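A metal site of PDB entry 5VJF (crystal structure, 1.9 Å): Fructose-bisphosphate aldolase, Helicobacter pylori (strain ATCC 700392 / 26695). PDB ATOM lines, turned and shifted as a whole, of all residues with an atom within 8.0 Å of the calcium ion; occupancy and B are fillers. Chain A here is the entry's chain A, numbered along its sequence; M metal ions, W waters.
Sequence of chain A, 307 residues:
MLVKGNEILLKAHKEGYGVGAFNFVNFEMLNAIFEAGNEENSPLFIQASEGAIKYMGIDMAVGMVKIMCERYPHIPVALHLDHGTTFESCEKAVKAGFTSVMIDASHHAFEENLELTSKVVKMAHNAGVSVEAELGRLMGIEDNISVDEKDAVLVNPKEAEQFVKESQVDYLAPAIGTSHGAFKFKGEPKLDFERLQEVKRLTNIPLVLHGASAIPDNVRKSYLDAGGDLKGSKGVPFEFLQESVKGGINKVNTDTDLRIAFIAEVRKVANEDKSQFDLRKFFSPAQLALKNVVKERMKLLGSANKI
The calcium ion is bound by water W1 (2.3 Å), OE1 of Glu 134 (2.3 Å), OD2 of Asp 104 (2.3 Å), OD1 of Asp 104 (2.4 Å), water W2 (2.5 Å), water W3 (2.5 Å) and OG of Ser 106 (2.5 Å).
Of the 19 residues printed, 3 come within 4 Å of the calcium ion.
The nearest printed residue that does not touch the calcium ion is His 83 (4.2 Å).
O of Ser 106 lies within hydrogen-bond range of NE of Arg 137 (3.0 Å).
N of Asp 104 sits at hydrogen-bond distance from O of Gly 84 (2.8 Å).
The side-chain hydroxyl (OG) of Ser 106 sits close to the backbone carbonyl oxygen (O) of Gly 136 (3.2 Å).
ND1 of His 83 lies close to OD2 of Asp 104 (2.8 Å).
The side-chain amide nitrogen (ND2) of Asn 113 lies within hydrogen-bond range of the backbone carbonyl oxygen (O) of Glu 134 (3.0 Å).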
ATOM      1  N   HIS A  83       1.456 -15.723 -27.568  1.00  0.00           N
ATOM      2  CA  HIS A  83       0.430 -16.452 -28.311  1.00  0.00           C
ATOM      3  C   HIS A  83       0.903 -17.097 -29.612  1.00  0.00           C
ATOM      4  O   HIS A  83       0.347 -16.843 -30.689  1.00  0.00           O
ATOM      5  CB  HIS A  83      -0.777 -15.543 -28.556  1.00  0.00           C
ATOM      6  CG  HIS A  83      -1.608 -15.330 -27.339  1.00  0.00           C
ATOM      7  ND1 HIS A  83      -2.560 -16.231 -26.929  1.00  0.00           N
ATOM      8  CD2 HIS A  83      -1.609 -14.336 -26.427  1.00  0.00           C
ATOM      9  CE1 HIS A  83      -3.131 -15.792 -25.812  1.00  0.00           C
ATOM     10  NE2 HIS A  83      -2.567 -14.642 -25.486  1.00  0.00           N
ATOM     11  N   GLY A  84       1.919 -17.944 -29.507  1.00  0.00           N
ATOM     12  CA  GLY A  84       2.287 -18.839 -30.576  1.00  0.00           C
ATOM     13  C   GLY A  84       1.106 -19.751 -30.859  1.00  0.00           C
ATOM     14  O   GLY A  84       0.475 -20.238 -29.924  1.00  0.00           O
ATOM     15  N   MET A 102       5.407 -18.930 -26.035  1.00  0.00           N
ATOM     16  CA  MET A 102       4.112 -19.417 -25.586  1.00  0.00           C
ATOM     17  C   MET A 102       3.460 -20.208 -26.702  1.00  0.00           C
ATOM     18  O   MET A 102       3.350 -19.726 -27.821  1.00  0.00           O
ATOM     19  CB  MET A 102       3.189 -18.266 -25.207  1.00  0.00           C
ATOM     20  CG  MET A 102       1.838 -18.763 -24.693  1.00  0.00           C
ATOM     21  SD  MET A 102       0.515 -17.571 -24.844  1.00  0.00           S
ATOM     22  CE  MET A 102      -0.815 -18.398 -23.981  1.00  0.00           C
ATOM     23  N   ILE A 103       3.030 -21.427 -26.384  1.00  0.00           N
ATOM     24  CA  ILE A 103       2.173 -22.161 -27.290  1.00  0.00           C
ATOM     25  C   ILE A 103       0.762 -22.105 -26.724  1.00  0.00           C
ATOM     26  O   ILE A 103       0.503 -22.587 -25.614  1.00  0.00           O
ATOM     27  CB  ILE A 103       2.654 -23.637 -27.490  1.00  0.00           C
ATOM     28  CG1 ILE A 103       1.679 -24.398 -28.405  1.00  0.00           C
ATOM     29  CG2 ILE A 103       2.802 -24.359 -26.164  1.00  0.00           C
ATOM     30  CD1 ILE A 103       1.575 -23.822 -29.812  1.00  0.00           C
ATOM     31  N   ASP A 104      -0.143 -21.480 -27.467  1.00  0.00           N
ATOM     32  CA  ASP A 104      -1.514 -21.334 -27.006  1.00  0.00           C
ATOM     33  C   ASP A 104      -2.438 -22.298 -27.730  1.00  0.00           C
ATOM     34  O   ASP A 104      -2.823 -22.080 -28.880  1.00  0.00           O
ATOM     35  CB  ASP A 104      -1.997 -19.895 -27.200  1.00  0.00           C
ATOM     36  CG  ASP A 104      -3.410 -19.687 -26.720  1.00  0.00           C
ATOM     37  OD1 ASP A 104      -3.981 -20.588 -26.062  1.00  0.00           O
ATOM     38  OD2 ASP A 104      -3.951 -18.604 -26.993  1.00  0.00           O
ATOM     39  N   ALA A 105      -2.781 -23.379 -27.038  1.00  0.00           N
ATOM     40  CA  ALA A 105      -3.718 -24.362 -27.551  1.00  0.00           C
ATOM     41  C   ALA A 105      -4.901 -24.521 -26.590  1.00  0.00           C
ATOM     42  O   ALA A 105      -5.531 -25.573 -26.542  1.00  0.00           O
ATOM     43  CB  ALA A 105      -3.008 -25.707 -27.722  1.00  0.00           C
ATOM     44  N   SER A 106      -5.214 -23.462 -25.844  1.00  0.00           N
ATOM     45  CA  SER A 106      -6.214 -23.537 -24.774  1.00  0.00           C
ATOM     46  C   SER A 106      -7.640 -23.708 -25.305  1.00  0.00           C
ATOM     47  O   SER A 106      -8.552 -24.072 -24.569  1.00  0.00           O
ATOM     48  CB  SER A 106      -6.157 -22.289 -23.883  1.00  0.00           C
ATOM     49  OG  SER A 106      -6.669 -21.149 -24.554  1.00  0.00           O
ATOM     50  N   HIS A 107      -7.830 -23.441 -26.586  1.00  0.00           N
ATOM     51  CA  HIS A 107      -9.130 -23.626 -27.222  1.00  0.00           C
ATOM     52  C   HIS A 107      -9.387 -25.102 -27.548  1.00  0.00           C
ATOM     53  O   HIS A 107     -10.509 -25.484 -27.863  1.00  0.00           O
ATOM     54  CB  HIS A 107      -9.242 -22.767 -28.481  1.00  0.00           C
ATOM     55  CG  HIS A 107      -8.205 -23.089 -29.512  1.00  0.00           C
ATOM     56  ND1 HIS A 107      -6.910 -22.636 -29.441  1.00  0.00           N
ATOM     57  CD2 HIS A 107      -8.277 -23.842 -30.641  1.00  0.00           C
ATOM     58  CE1 HIS A 107      -6.232 -23.080 -30.477  1.00  0.00           C
ATOM     59  NE2 HIS A 107      -7.032 -23.820 -31.220  1.00  0.00           N
ATOM     60  N   HIS A 108      -8.347 -25.933 -27.474  1.00  0.00           N
ATOM     61  CA  HIS A 108      -8.507 -27.359 -27.697  1.00  0.00           C
ATOM     62  C   HIS A 108      -8.897 -28.060 -26.410  1.00  0.00           C
ATOM     63  O   HIS A 108      -8.742 -27.517 -25.317  1.00  0.00           O
ATOM     64  CB  HIS A 108      -7.213 -27.975 -28.227  1.00  0.00           C
ATOM     65  CG  HIS A 108      -6.912 -27.641 -29.648  1.00  0.00           C
ATOM     66  ND1 HIS A 108      -7.897 -27.504 -30.607  1.00  0.00           N
ATOM     67  CD2 HIS A 108      -5.742 -27.379 -30.272  1.00  0.00           C
ATOM     68  CE1 HIS A 108      -7.331 -27.195 -31.768  1.00  0.00           C
ATOM     69  NE2 HIS A 108      -6.027 -27.107 -31.591  1.00  0.00           N
ATOM     70  N   ASN A 113      -4.380 -30.064 -26.290  1.00  0.00           N
ATOM     71  CA  ASN A 113      -3.559 -28.985 -25.711  1.00  0.00           C
ATOM     72  C   ASN A 113      -2.278 -29.584 -25.148  1.00  0.00           C
ATOM     73  O   ASN A 113      -1.163 -29.126 -25.433  1.00  0.00           O
ATOM     74  CB  ASN A 113      -4.372 -28.249 -24.640  1.00  0.00           C
ATOM     75  CG  ASN A 113      -3.669 -27.009 -24.093  1.00  0.00           C
ATOM     76  OD1 ASN A 113      -2.564 -26.650 -24.502  1.00  0.00           O
ATOM     77  ND2 ASN A 113      -4.336 -26.326 -23.173  1.00  0.00           N
ATOM     78  N   ALA A 133       2.307 -22.164 -21.538  1.00  0.00           N
ATOM     79  CA  ALA A 133       1.081 -22.674 -22.141  1.00  0.00           C
ATOM     80  C   ALA A 133      -0.117 -22.114 -21.387  1.00  0.00           C
ATOM     81  O   ALA A 133       0.041 -21.463 -20.357  1.00  0.00           O
ATOM     82  CB  ALA A 133       1.078 -24.207 -22.148  1.00  0.00           C
ATOM     83  N   GLU A 134      -1.317 -22.364 -21.892  1.00  0.00           N
ATOM     84  CA  GLU A 134      -2.509 -21.745 -21.344  1.00  0.00           C
ATOM     85  C   GLU A 134      -3.590 -22.791 -21.105  1.00  0.00           C
ATOM     86  O   GLU A 134      -3.748 -23.735 -21.882  1.00  0.00           O
ATOM     87  CB  GLU A 134      -3.013 -20.628 -22.262  1.00  0.00           C
ATOM     88  CG  GLU A 134      -4.236 -19.879 -21.727  1.00  0.00           C
ATOM     89  CD  GLU A 134      -4.498 -18.579 -22.492  1.00  0.00           C
ATOM     90  OE1 GLU A 134      -4.748 -18.636 -23.712  1.00  0.00           O
ATOM     91  OE2 GLU A 134      -4.457 -17.490 -21.871  1.00  0.00           O
ATOM     92  N   LEU A 135      -4.321 -22.611 -20.020  1.00  0.00           N
ATOM     93  CA  LEU A 135      -5.422 -23.513 -19.682  1.00  0.00           C
ATOM     94  C   LEU A 135      -6.640 -22.672 -19.299  1.00  0.00           C
ATOM     95  O   LEU A 135      -6.545 -21.766 -18.461  1.00  0.00           O
ATOM     96  CB  LEU A 135      -4.992 -24.425 -18.534  1.00  0.00           C
ATOM     97  CG  LEU A 135      -5.437 -25.871 -18.423  1.00  0.00           C
ATOM     98  CD1 LEU A 135      -5.493 -26.551 -19.770  1.00  0.00           C
ATOM     99  CD2 LEU A 135      -4.461 -26.586 -17.499  1.00  0.00           C
ATOM    100  N   GLY A 136      -7.771 -22.981 -19.920  1.00  0.00           N
ATOM    101  CA  GLY A 136      -8.977 -22.192 -19.744  1.00  0.00           C
ATOM    102  C   GLY A 136      -9.203 -21.270 -20.920  1.00  0.00           C
ATOM    103  O   GLY A 136      -8.335 -21.122 -21.771  1.00  0.00           O
ATOM    104  N   ARG A 137     -10.359 -20.618 -20.967  1.00  0.00           N
ATOM    105  CA  ARG A 137     -10.689 -19.739 -22.087  1.00  0.00           C
ATOM    106  C   ARG A 137     -11.075 -18.336 -21.630  1.00  0.00           C
ATOM    107  O   ARG A 137     -12.116 -18.124 -21.010  1.00  0.00           O
ATOM    108  CB  ARG A 137     -11.806 -20.354 -22.931  1.00  0.00           C
ATOM    109  CG  ARG A 137     -11.293 -21.441 -23.876  1.00  0.00           C
ATOM    110  CD  ARG A 137     -12.221 -22.635 -23.943  1.00  0.00           C
ATOM    111  NE  ARG A 137     -11.494 -23.853 -24.267  1.00  0.00           N
ATOM    112  CZ  ARG A 137     -12.039 -25.061 -24.348  1.00  0.00           C
ATOM    113  NH1 ARG A 137     -13.338 -25.228 -24.140  1.00  0.00           N
ATOM    114  NH2 ARG A 137     -11.276 -26.109 -24.636  1.00  0.00           N
ATOM    115  N   LEU A 138     -10.206 -17.362 -21.938  1.00  0.00           N
ATOM    116  CA  LEU A 138     -10.512 -15.951 -21.736  1.00  0.00           C
ATOM    117  C   LEU A 138     -11.638 -15.531 -22.676  1.00  0.00           C
ATOM    118  O   LEU A 138     -11.520 -15.658 -23.895  1.00  0.00           O
ATOM    119  CB  LEU A 138      -9.269 -15.090 -21.986  1.00  0.00           C
ATOM    120  CG  LEU A 138      -8.303 -14.908 -20.811  1.00  0.00           C
ATOM    121  CD1 LEU A 138      -7.872 -16.231 -20.211  1.00  0.00           C
ATOM    122  CD2 LEU A 138      -7.099 -14.085 -21.242  1.00  0.00           C
ATOM    123  N   ALA A 173      -0.379 -20.126 -17.909  1.00  0.00           N
ATOM    124  CA  ALA A 173      -1.369 -19.052 -17.849  1.00  0.00           C
ATOM    125  C   ALA A 173      -2.745 -19.635 -17.544  1.00  0.00           C
ATOM    126  O   ALA A 173      -3.410 -20.168 -18.423  1.00  0.00           O
ATOM    127  CB  ALA A 173      -1.417 -18.329 -19.178  1.00  0.00           C
ATOM    128  N   HIS A 180      -8.378 -10.185 -22.900  1.00  0.00           N
ATOM    129  CA  HIS A 180      -7.563  -9.217 -23.610  1.00  0.00           C
ATOM    130  C   HIS A 180      -8.359  -7.959 -23.891  1.00  0.00           C
ATOM    131  O   HIS A 180      -9.576  -8.010 -24.038  1.00  0.00           O
ATOM    132  CB  HIS A 180      -7.086  -9.788 -24.943  1.00  0.00           C
ATOM    133  CG  HIS A 180      -5.966 -10.767 -24.818  1.00  0.00           C
ATOM    134  ND1 HIS A 180      -4.824 -10.683 -25.585  1.00  0.00           N
ATOM    135  CD2 HIS A 180      -5.811 -11.839 -24.016  1.00  0.00           C
ATOM    136  CE1 HIS A 180      -4.017 -11.685 -25.259  1.00  0.00           C
ATOM    137  NE2 HIS A 180      -4.586 -12.395 -24.307  1.00  0.00           N
ATOM    138  N   HIS A 210      -2.688 -13.265 -18.268  1.00  0.00           N
ATOM    139  CA  HIS A 210      -2.994 -12.577 -19.522  1.00  0.00           C
ATOM    140  C   HIS A 210      -4.084 -11.539 -19.291  1.00  0.00           C
ATOM    141  O   HIS A 210      -4.798 -11.592 -18.288  1.00  0.00           O
ATOM    142  CB  HIS A 210      -3.410 -13.570 -20.606  1.00  0.00           C
ATOM    143  CG  HIS A 210      -2.277 -14.375 -21.159  1.00  0.00           C
ATOM    144  ND1 HIS A 210      -1.961 -14.397 -22.494  1.00  0.00           N
ATOM    145  CD2 HIS A 210      -1.356 -15.150 -20.544  1.00  0.00           C
ATOM    146  CE1 HIS A 210      -0.917 -15.173 -22.685  1.00  0.00           C
ATOM    147  NE2 HIS A 210      -0.533 -15.649 -21.522  1.00  0.00           N
HETATM  148 CA    CA M   1      -5.811 -19.074 -25.702  1.00  0.00          CA
HETATM  149 ZN    ZN M   2      -3.159 -13.648 -23.896  1.00  0.00          ZN
HETATM  150  O   HOH W   1      -6.201 -16.886 -26.151  1.00  0.00           O
HETATM  151  O   HOH W   2      -7.988 -18.507 -24.725  1.00  0.00           O
HETATM  152  O   HOH W   3      -6.680 -19.961 -27.845  1.00  0.00           O
